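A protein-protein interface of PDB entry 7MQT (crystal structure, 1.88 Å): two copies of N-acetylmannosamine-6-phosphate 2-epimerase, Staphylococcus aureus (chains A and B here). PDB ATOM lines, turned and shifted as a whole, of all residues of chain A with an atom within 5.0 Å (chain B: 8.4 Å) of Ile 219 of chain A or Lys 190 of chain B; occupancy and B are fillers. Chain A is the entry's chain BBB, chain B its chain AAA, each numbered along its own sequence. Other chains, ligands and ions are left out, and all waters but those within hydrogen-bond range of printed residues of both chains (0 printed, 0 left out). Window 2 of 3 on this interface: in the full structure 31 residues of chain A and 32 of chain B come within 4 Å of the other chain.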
ATOM      1  N   ARG A 215      17.549  19.099 -27.577  1.00  0.00           N
ATOM      2  CA  ARG A 215      17.739  19.110 -26.106  1.00  0.00           C
ATOM      3  C   ARG A 215      16.930  17.959 -25.473  1.00  0.00           C
ATOM      4  O   ARG A 215      17.423  17.348 -24.519  1.00  0.00           O
ATOM      5  CB  ARG A 215      17.346  20.475 -25.544  1.00  0.00           C
ATOM      6  CG  ARG A 215      18.227  21.607 -26.044  1.00  0.00           C
ATOM      7  CD  ARG A 215      18.101  22.863 -25.194  1.00  0.00           C
ATOM      8  NE  ARG A 215      16.944  23.662 -25.552  1.00  0.00           N
ATOM      9  CZ  ARG A 215      15.884  23.906 -24.762  1.00  0.00           C
ATOM     10  NH1 ARG A 215      15.795  23.415 -23.536  1.00  0.00           N
ATOM     11  NH2 ARG A 215      14.914  24.686 -25.200  1.00  0.00           N
ATOM     12  N   PHE A 216      15.746  17.667 -25.988  1.00  0.00           N
ATOM     13  CA  PHE A 216      14.968  16.502 -25.494  1.00  0.00           C
ATOM     14  C   PHE A 216      15.761  15.235 -25.799  1.00  0.00           C
ATOM     15  O   PHE A 216      15.914  14.432 -24.908  1.00  0.00           O
ATOM     16  CB  PHE A 216      13.569  16.412 -26.096  1.00  0.00           C
ATOM     17  CG  PHE A 216      12.546  17.229 -25.352  1.00  0.00           C
ATOM     18  CD1 PHE A 216      12.466  18.592 -25.538  1.00  0.00           C
ATOM     19  CD2 PHE A 216      11.684  16.641 -24.442  1.00  0.00           C
ATOM     20  CE1 PHE A 216      11.537  19.357 -24.841  1.00  0.00           C
ATOM     21  CE2 PHE A 216      10.736  17.397 -23.776  1.00  0.00           C
ATOM     22  CZ  PHE A 216      10.691  18.752 -23.946  1.00  0.00           C
ATOM     23  N   VAL A 217      16.152  15.022 -27.052  1.00  0.00           N
ATOM     24  CA  VAL A 217      16.906  13.797 -27.455  1.00  0.00           C
ATOM     25  C   VAL A 217      18.163  13.716 -26.596  1.00  0.00           C
ATOM     26  O   VAL A 217      18.501  12.638 -26.139  1.00  0.00           O
ATOM     27  CB  VAL A 217      17.239  13.811 -28.959  1.00  0.00           C
ATOM     28  CG1 VAL A 217      18.156  12.660 -29.367  1.00  0.00           C
ATOM     29  CG2 VAL A 217      15.998  13.786 -29.818  1.00  0.00           C
ATOM     30  N   GLN A 218      18.843  14.832 -26.366  1.00  0.00           N
ATOM     31  CA  GLN A 218      20.197  14.823 -25.760  1.00  0.00           C
ATOM     32  C   GLN A 218      20.123  14.258 -24.337  1.00  0.00           C
ATOM     33  O   GLN A 218      21.096  13.697 -23.865  1.00  0.00           O
ATOM     34  CB  GLN A 218      20.806  16.225 -25.740  1.00  0.00           C
ATOM     35  CG  GLN A 218      22.146  16.311 -25.009  1.00  0.00           C
ATOM     36  CD  GLN A 218      23.215  15.454 -25.659  1.00  0.00           C
ATOM     37  OE1 GLN A 218      23.329  15.424 -26.885  1.00  0.00           O
ATOM     38  NE2 GLN A 218      23.972  14.695 -24.859  1.00  0.00           N
ATOM     39  N   ILE A 219      19.028  14.473 -23.621  1.00  0.00           N
ATOM     40  CA  ILE A 219      18.975  14.033 -22.204  1.00  0.00           C
ATOM     41  C   ILE A 219      18.951  12.502 -22.158  1.00  0.00           C
ATOM     42  O   ILE A 219      19.166  11.979 -21.063  1.00  0.00           O
ATOM     43  CB  ILE A 219      17.791  14.648 -21.438  1.00  0.00           C
ATOM     44  CG1 ILE A 219      18.110  14.724 -19.937  1.00  0.00           C
ATOM     45  CG2 ILE A 219      16.503  13.897 -21.740  1.00  0.00           C
ATOM     46  CD1 ILE A 219      17.098  15.483 -19.118  1.00  0.00           C
ATOM     47  N   MET A 220      18.643  11.824 -23.276  1.00  0.00           N
ATOM     48  CA  MET A 220      18.659  10.346 -23.360  1.00  0.00           C
ATOM     49  C   MET A 220      20.042   9.862 -23.816  1.00  0.00           C
ATOM     50  O   MET A 220      20.279   8.623 -23.816  1.00  0.00           O
ATOM     51  CB  MET A 220      17.590   9.849 -24.339  1.00  0.00           C
ATOM     52  CG  MET A 220      16.172  10.164 -23.914  1.00  0.00           C
ATOM     53  SD  MET A 220      15.815   9.711 -22.208  1.00  0.00           S
ATOM     54  CE  MET A 220      16.093   7.949 -22.321  1.00  0.00           C
ATOM     55  N   GLU A 221      20.942  10.769 -24.181  1.00  0.00           N
ATOM     56  CA  GLU A 221      22.232  10.389 -24.818  1.00  0.00           C
ATOM     57  C   GLU A 221      23.408  10.663 -23.874  1.00  0.00           C
ATOM     58  O   GLU A 221      24.461  10.068 -24.110  1.00  0.00           O
ATOM     59  CB  GLU A 221      22.427  11.132 -26.136  1.00  0.00           C
ATOM     60  CG  GLU A 221      21.317  10.918 -27.158  1.00  0.00           C
ATOM     61  CD  GLU A 221      21.157   9.498 -27.678  1.00  0.00           C
ATOM     62  OE1 GLU A 221      22.080   8.674 -27.471  1.00  0.00           O
ATOM     63  OE2 GLU A 221      20.116   9.233 -28.321  1.00  0.00           O
ATOM     64  N   ASP A 222      23.246  11.545 -22.884  1.00  0.00           N
ATOM     65  CA  ASP A 222      24.267  11.821 -21.832  1.00  0.00           C
ATOM     66  C   ASP A 222      24.685  10.503 -21.183  1.00  0.00           C
ATOM     67  O   ASP A 222      23.799   9.750 -20.779  1.00  0.00           O
ATOM     68  CB  ASP A 222      23.745  12.739 -20.726  1.00  0.00           C
ATOM     69  CG  ASP A 222      23.262  14.082 -21.239  1.00  0.00           C
ATOM     70  OD1 ASP A 222      23.843  14.570 -22.241  1.00  0.00           O
ATOM     71  OD2 ASP A 222      22.315  14.631 -20.621  1.00  0.00           O
ATOM     72  OXT ASP A 222      25.878  10.206 -21.073  1.00  0.00           O
ATOM     73  N   LEU B   6      11.686   9.730 -29.085  1.00  0.00           N
ATOM     74  CA  LEU B   6      10.882  10.958 -29.023  1.00  0.00           C
ATOM     75  C   LEU B   6      10.034  11.050 -30.269  1.00  0.00           C
ATOM     76  O   LEU B   6      10.567  11.111 -31.379  1.00  0.00           O
ATOM     77  CB  LEU B   6      11.797  12.170 -28.872  1.00  0.00           C
ATOM     78  CG  LEU B   6      11.053  13.509 -28.772  1.00  0.00           C
ATOM     79  CD1 LEU B   6      10.329  13.601 -27.426  1.00  0.00           C
ATOM     80  CD2 LEU B   6      12.008  14.676 -28.906  1.00  0.00           C
ATOM     81  N   PHE B 163       4.731  11.066 -11.565  1.00  0.00           N
ATOM     82  CA  PHE B 163       4.209  10.244 -12.694  1.00  0.00           C
ATOM     83  C   PHE B 163       3.472   9.014 -12.156  1.00  0.00           C
ATOM     84  O   PHE B 163       3.461   7.978 -12.816  1.00  0.00           O
ATOM     85  CB  PHE B 163       5.360   9.898 -13.639  1.00  0.00           C
ATOM     86  CG  PHE B 163       5.872  11.095 -14.388  1.00  0.00           C
ATOM     87  CD1 PHE B 163       5.235  11.528 -15.535  1.00  0.00           C
ATOM     88  CD2 PHE B 163       6.917  11.846 -13.887  1.00  0.00           C
ATOM     89  CE1 PHE B 163       5.683  12.633 -16.235  1.00  0.00           C
ATOM     90  CE2 PHE B 163       7.359  12.976 -14.576  1.00  0.00           C
ATOM     91  CZ  PHE B 163       6.730  13.369 -15.737  1.00  0.00           C
ATOM     92  N   VAL B 183       4.226  16.258 -21.101  1.00  0.00           N
ATOM     93  CA  VAL B 183       5.684  15.985 -21.065  1.00  0.00           C
ATOM     94  C   VAL B 183       6.321  17.286 -21.542  1.00  0.00           C
ATOM     95  O   VAL B 183       6.383  17.496 -22.749  1.00  0.00           O
ATOM     96  CB  VAL B 183       6.104  14.768 -21.895  1.00  0.00           C
ATOM     97  CG1 VAL B 183       7.581  14.483 -21.700  1.00  0.00           C
ATOM     98  CG2 VAL B 183       5.273  13.545 -21.511  1.00  0.00           C
ATOM     99  N   THR B 185       9.318  19.049 -20.368  1.00  0.00           N
ATOM    100  CA  THR B 185      10.769  19.326 -20.286  1.00  0.00           C
ATOM    101  C   THR B 185      11.520  18.052 -20.646  1.00  0.00           C
ATOM    102  O   THR B 185      10.973  16.963 -20.446  1.00  0.00           O
ATOM    103  CB  THR B 185      11.188  19.783 -18.881  1.00  0.00           C
ATOM    104  OG1 THR B 185      10.998  18.683 -17.985  1.00  0.00           O
ATOM    105  CG2 THR B 185      10.409  20.985 -18.397  1.00  0.00           C
ATOM    106  N   PRO B 186      12.793  18.188 -21.095  1.00  0.00           N
ATOM    107  CA  PRO B 186      13.739  17.075 -21.190  1.00  0.00           C
ATOM    108  C   PRO B 186      13.786  16.241 -19.913  1.00  0.00           C
ATOM    109  O   PRO B 186      13.801  15.053 -20.029  1.00  0.00           O
ATOM    110  CB  PRO B 186      15.066  17.777 -21.491  1.00  0.00           C
ATOM    111  CG  PRO B 186      14.603  18.988 -22.289  1.00  0.00           C
ATOM    112  CD  PRO B 186      13.395  19.461 -21.536  1.00  0.00           C
ATOM    113  N   ASP B 187      13.741  16.855 -18.725  1.00  0.00           N
ATOM    114  CA  ASP B 187      13.819  16.087 -17.461  1.00  0.00           C
ATOM    115  C   ASP B 187      12.610  15.140 -17.371  1.00  0.00           C
ATOM    116  O   ASP B 187      12.767  14.009 -16.959  1.00  0.00           O
ATOM    117  CB  ASP B 187      13.869  17.013 -16.252  1.00  0.00           C
ATOM    118  CG  ASP B 187      15.222  17.642 -15.979  1.00  0.00           C
ATOM    119  OD1 ASP B 187      16.274  17.071 -16.425  1.00  0.00           O
ATOM    120  OD2 ASP B 187      15.212  18.688 -15.297  1.00  0.00           O
ATOM    121  N   MET B 188      11.413  15.635 -17.680  1.00  0.00           N
ATOM    122  CA  MET B 188      10.168  14.825 -17.699  1.00  0.00           C
ATOM    123  C   MET B 188      10.302  13.708 -18.733  1.00  0.00           C
ATOM    124  O   MET B 188       9.924  12.576 -18.439  1.00  0.00           O
ATOM    125  CB  MET B 188       8.941  15.676 -18.027  1.00  0.00           C
ATOM    126  CG  MET B 188       8.490  16.514 -16.854  1.00  0.00           C
ATOM    127  SD  MET B 188       6.906  17.218 -17.231  1.00  0.00           S
ATOM    128  CE  MET B 188       6.834  18.494 -15.968  1.00  0.00           C
ATOM    129  N   TYR B 189      10.855  14.010 -19.903  1.00  0.00           N
ATOM    130  CA  TYR B 189      11.016  13.008 -20.981  1.00  0.00           C
ATOM    131  C   TYR B 189      11.939  11.919 -20.464  1.00  0.00           C
ATOM    132  O   TYR B 189      11.611  10.723 -20.558  1.00  0.00           O
ATOM    133  CB  TYR B 189      11.530  13.671 -22.258  1.00  0.00           C
ATOM    134  CG  TYR B 189      11.972  12.716 -23.331  1.00  0.00           C
ATOM    135  CD1 TYR B 189      11.161  11.670 -23.725  1.00  0.00           C
ATOM    136  CD2 TYR B 189      13.156  12.913 -24.011  1.00  0.00           C
ATOM    137  CE1 TYR B 189      11.558  10.783 -24.703  1.00  0.00           C
ATOM    138  CE2 TYR B 189      13.551  12.069 -25.021  1.00  0.00           C
ATOM    139  CZ  TYR B 189      12.763  10.980 -25.337  1.00  0.00           C
ATOM    140  OH  TYR B 189      13.198  10.104 -26.259  1.00  0.00           O
ATOM    141  N   LYS B 190      13.052  12.307 -19.866  1.00  0.00           N
ATOM    142  CA  LYS B 190      13.992  11.314 -19.293  1.00  0.00           C
ATOM    143  C   LYS B 190      13.276  10.472 -18.231  1.00  0.00           C
ATOM    144  O   LYS B 190      13.472   9.278 -18.190  1.00  0.00           O
ATOM    145  CB  LYS B 190      15.190  11.956 -18.593  1.00  0.00           C
ATOM    146  CG  LYS B 190      16.174  10.910 -18.075  1.00  0.00           C
ATOM    147  CD  LYS B 190      17.475  11.466 -17.555  1.00  0.00           C
ATOM    148  CE  LYS B 190      18.124  10.587 -16.497  1.00  0.00           C
ATOM    149  NZ  LYS B 190      18.434   9.277 -17.078  1.00  0.00           N
ATOM    150  N   ARG B 191      12.487  11.101 -17.365  1.00  0.00           N
ATOM    151  CA  ARG B 191      11.829  10.375 -16.253  1.00  0.00           C
ATOM    152  C   ARG B 191      10.875   9.316 -16.841  1.00  0.00           C
ATOM    153  O   ARG B 191      10.951   8.120 -16.414  1.00  0.00           O
ATOM    154  CB  ARG B 191      11.131  11.380 -15.340  1.00  0.00           C
ATOM    155  CG  ARG B 191      10.508  10.747 -14.116  1.00  0.00           C
ATOM    156  CD  ARG B 191      11.520  10.512 -13.025  1.00  0.00           C
ATOM    157  NE  ARG B 191      10.957   9.691 -11.964  1.00  0.00           N
ATOM    158  CZ  ARG B 191      11.370   8.459 -11.635  1.00  0.00           C
ATOM    159  NH1 ARG B 191      12.349   7.858 -12.291  1.00  0.00           N
ATOM    160  NH2 ARG B 191      10.802   7.819 -10.633  1.00  0.00           N
ATOM    161  N   VAL B 192      10.030   9.689 -17.807  1.00  0.00           N
ATOM    162  CA  VAL B 192       9.034   8.725 -18.374  1.00  0.00           C
ATOM    163  C   VAL B 192       9.749   7.584 -19.080  1.00  0.00           C
ATOM    164  O   VAL B 192       9.292   6.424 -18.925  1.00  0.00           O
ATOM    165  CB  VAL B 192       7.967   9.366 -19.262  1.00  0.00           C
ATOM    166  CG1 VAL B 192       7.205  10.397 -18.444  1.00  0.00           C
ATOM    167  CG2 VAL B 192       8.520   9.953 -20.539  1.00  0.00           C
ATOM    168  N   MET B 193      10.811   7.889 -19.810  1.00  0.00           N
ATOM    169  CA  MET B 193      11.637   6.853 -20.459  1.00  0.00           C
ATOM    170  C   MET B 193      12.253   5.943 -19.395  1.00  0.00           C
ATOM    171  O   MET B 193      12.144   4.736 -19.559  1.00  0.00           O
ATOM    172  CB  MET B 193      12.691   7.463 -21.392  1.00  0.00           C
ATOM    173  CG  MET B 193      12.044   8.203 -22.529  1.00  0.00           C
ATOM    174  SD  MET B 193      11.083   7.211 -23.667  1.00  0.00           S
ATOM    175  CE  MET B 193      12.412   6.759 -24.773  1.00  0.00           C
ATOM    176  N   ASP B 194      12.821   6.484 -18.324  1.00  0.00           N
ATOM    177  CA  ASP B 194      13.432   5.639 -17.269  1.00  0.00           C
ATOM    178  C   ASP B 194      12.354   4.793 -16.598  1.00  0.00           C
ATOM    179  O   ASP B 194      12.690   3.722 -16.134  1.00  0.00           O
ATOM    180  CB  ASP B 194      14.158   6.469 -16.223  1.00  0.00           C
ATOM    181  CG  ASP B 194      15.425   7.101 -16.741  1.00  0.00           C
ATOM    182  OD1 ASP B 194      15.845   6.780 -17.862  1.00  0.00           O
ATOM    183  OD2 ASP B 194      15.928   7.996 -16.033  1.00  0.00           O
ATOM    184  N   LEU B 195      11.113   5.257 -16.524  1.00  0.00           N
ATOM    185  CA  LEU B 195      10.009   4.485 -15.917  1.00  0.00           C
ATOM    186  C   LEU B 195       9.586   3.339 -16.831  1.00  0.00           C
ATOM    187  O   LEU B 195       8.914   2.465 -16.300  1.00  0.00           O
ATOM    188  CB  LEU B 195       8.845   5.420 -15.576  1.00  0.00           C
ATOM    189  CG  LEU B 195       9.131   6.349 -14.392  1.00  0.00           C
ATOM    190  CD1 LEU B 195       7.995   7.317 -14.145  1.00  0.00           C
ATOM    191  CD2 LEU B 195       9.403   5.528 -13.134  1.00  0.00           C
ATOM    192  N   GLY B 196       9.952   3.337 -18.115  1.00  0.00           N
ATOM    193  CA  GLY B 196       9.775   2.164 -19.003  1.00  0.00           C
ATOM    194  C   GLY B 196       8.760   2.369 -20.113  1.00  0.00           C
ATOM    195  O   GLY B 196       8.290   1.384 -20.693  1.00  0.00           O
ATOM    196  N   VAL B 197       8.365   3.597 -20.409  1.00  0.00           N
ATOM    197  CA  VAL B 197       7.446   3.805 -21.561  1.00  0.00           C
ATOM    198  C   VAL B 197       8.206   3.374 -22.808  1.00  0.00           C
ATOM    199  O   VAL B 197       9.436   3.453 -22.819  1.00  0.00           O
ATOM    200  CB  VAL B 197       6.917   5.240 -21.691  1.00  0.00           C
ATOM    201  CG1 VAL B 197       6.182   5.654 -20.437  1.00  0.00           C
ATOM    202  CG2 VAL B 197       8.018   6.235 -22.031  1.00  0.00           C
ATOM    203  N   SER B 200       7.777   8.561 -25.980  1.00  0.00           N
ATOM    204  CA  SER B 200       7.044   9.732 -25.456  1.00  0.00           C
ATOM    205  C   SER B 200       6.667  10.647 -26.616  1.00  0.00           C
ATOM    206  O   SER B 200       7.443  10.755 -27.534  1.00  0.00           O
ATOM    207  CB  SER B 200       7.867  10.462 -24.399  1.00  0.00           C
ATOM    208  OG  SER B 200       7.141  11.552 -23.869  1.00  0.00           O
ATOM    209  N   VAL B 202       5.889  14.451 -27.351  1.00  0.00           N
ATOM    210  CA  VAL B 202       6.022  15.843 -26.870  1.00  0.00           C
ATOM    211  C   VAL B 202       5.456  16.758 -27.958  1.00  0.00           C
ATOM    212  O   VAL B 202       5.835  16.633 -29.160  1.00  0.00           O
ATOM    213  CB  VAL B 202       7.488  16.114 -26.539  1.00  0.00           C
ATOM    214  CG1 VAL B 202       7.706  17.588 -26.260  1.00  0.00           C
ATOM    215  CG2 VAL B 202       7.944  15.247 -25.390  1.00  0.00           C
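Of the 8 printed residues of chain A, 4 touch a printed residue of chain B.
N of Leu 6 of chain B sits at hydrogen-bond distance from OH of Tyr 189 of chain B, at 3.2 Å.
OG1 of Thr 185 of chain B sits close to N of Asp 187 of chain B (3.4 Å).
The backbone NH (N) of Met 188 of chain B sits at hydrogen-bond distance from the side-chain hydroxyl (OG1) of Thr 185 of chain B.
NZ of Lys 190 of chain B lies within salt-bridge range of OD2 of Asp 194 of chain B, 3.0 Å away.
Among the printed residues, merely in contact across the chains: Arg 215 of chain A with Pro 186 of chain B (3.9 Å), Phe 216 of chain A with Leu 6 of chain B (3.7 Å), Phe 216 of chain A with Thr 185 of chain B (3.3 Å), Phe 216 of chain A with Pro 186 of chain B (3.5 Å), Phe 216 of chain A with Tyr 189 of chain B (3.3 Å), Phe 216 of chain A with Val 202 of chain B (3.9 Å), Ile 219 of chain A with Pro 186 of chain B (3.4 Å), Ile 219 of chain A with Asp 187 of chain B (3.2 Å), Ile 219 of chain A with Lys 190 of chain B (3.9 Å), Met 220 of chain A with Tyr 189 of chain B (3.4 Å), Met 220 of chain A with Lys 190 of chain B (3.8 Å) and Met 220 of chain A with Met 193 of chain B (3.6 Å).
Of the printed residues of chain B, Ile 219 of chain A touches Pro 186 (3.4 Å), Asp 187 (3.2 Å) and Lys 190 (3.9 Å).
Of the printed residues of chain A, Lys 190 of chain B touches Ile 219 (3.9 Å) and Met 220 (3.8 Å).
Of the printed residues of chain B, Met 220 of chain A touches Tyr 189, Lys 190 and Met 193.
Of the printed residues of chain A, Leu 6 of chain B touches Phe 216 (3.7 Å).
Of the printed residues of chain B, Phe 216 of chain A touches Leu 6 (3.7 Å), Thr 185 (3.3 Å), Pro 186 (3.5 Å), Tyr 189 (3.3 Å) and Val 202 (3.9 Å).
Arg 191 of chain B touches none of the printed residues of chain A.
Asp 194 of chain B touches none of the printed residues of chain A.
The nearest printed residue of chain B that does not touch Ile 219 of chain A is Tyr 189 of chain B (4.2 Å).
The nearest printed residue of chain A that does not touch Lys 190 of chain B is Phe 216 of chain A (6.2 Å).
No position is printed for both chains.
Of the 12 pairs that touch across the chains among the printed residues, none has its exchanged pair printed and touching as well.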
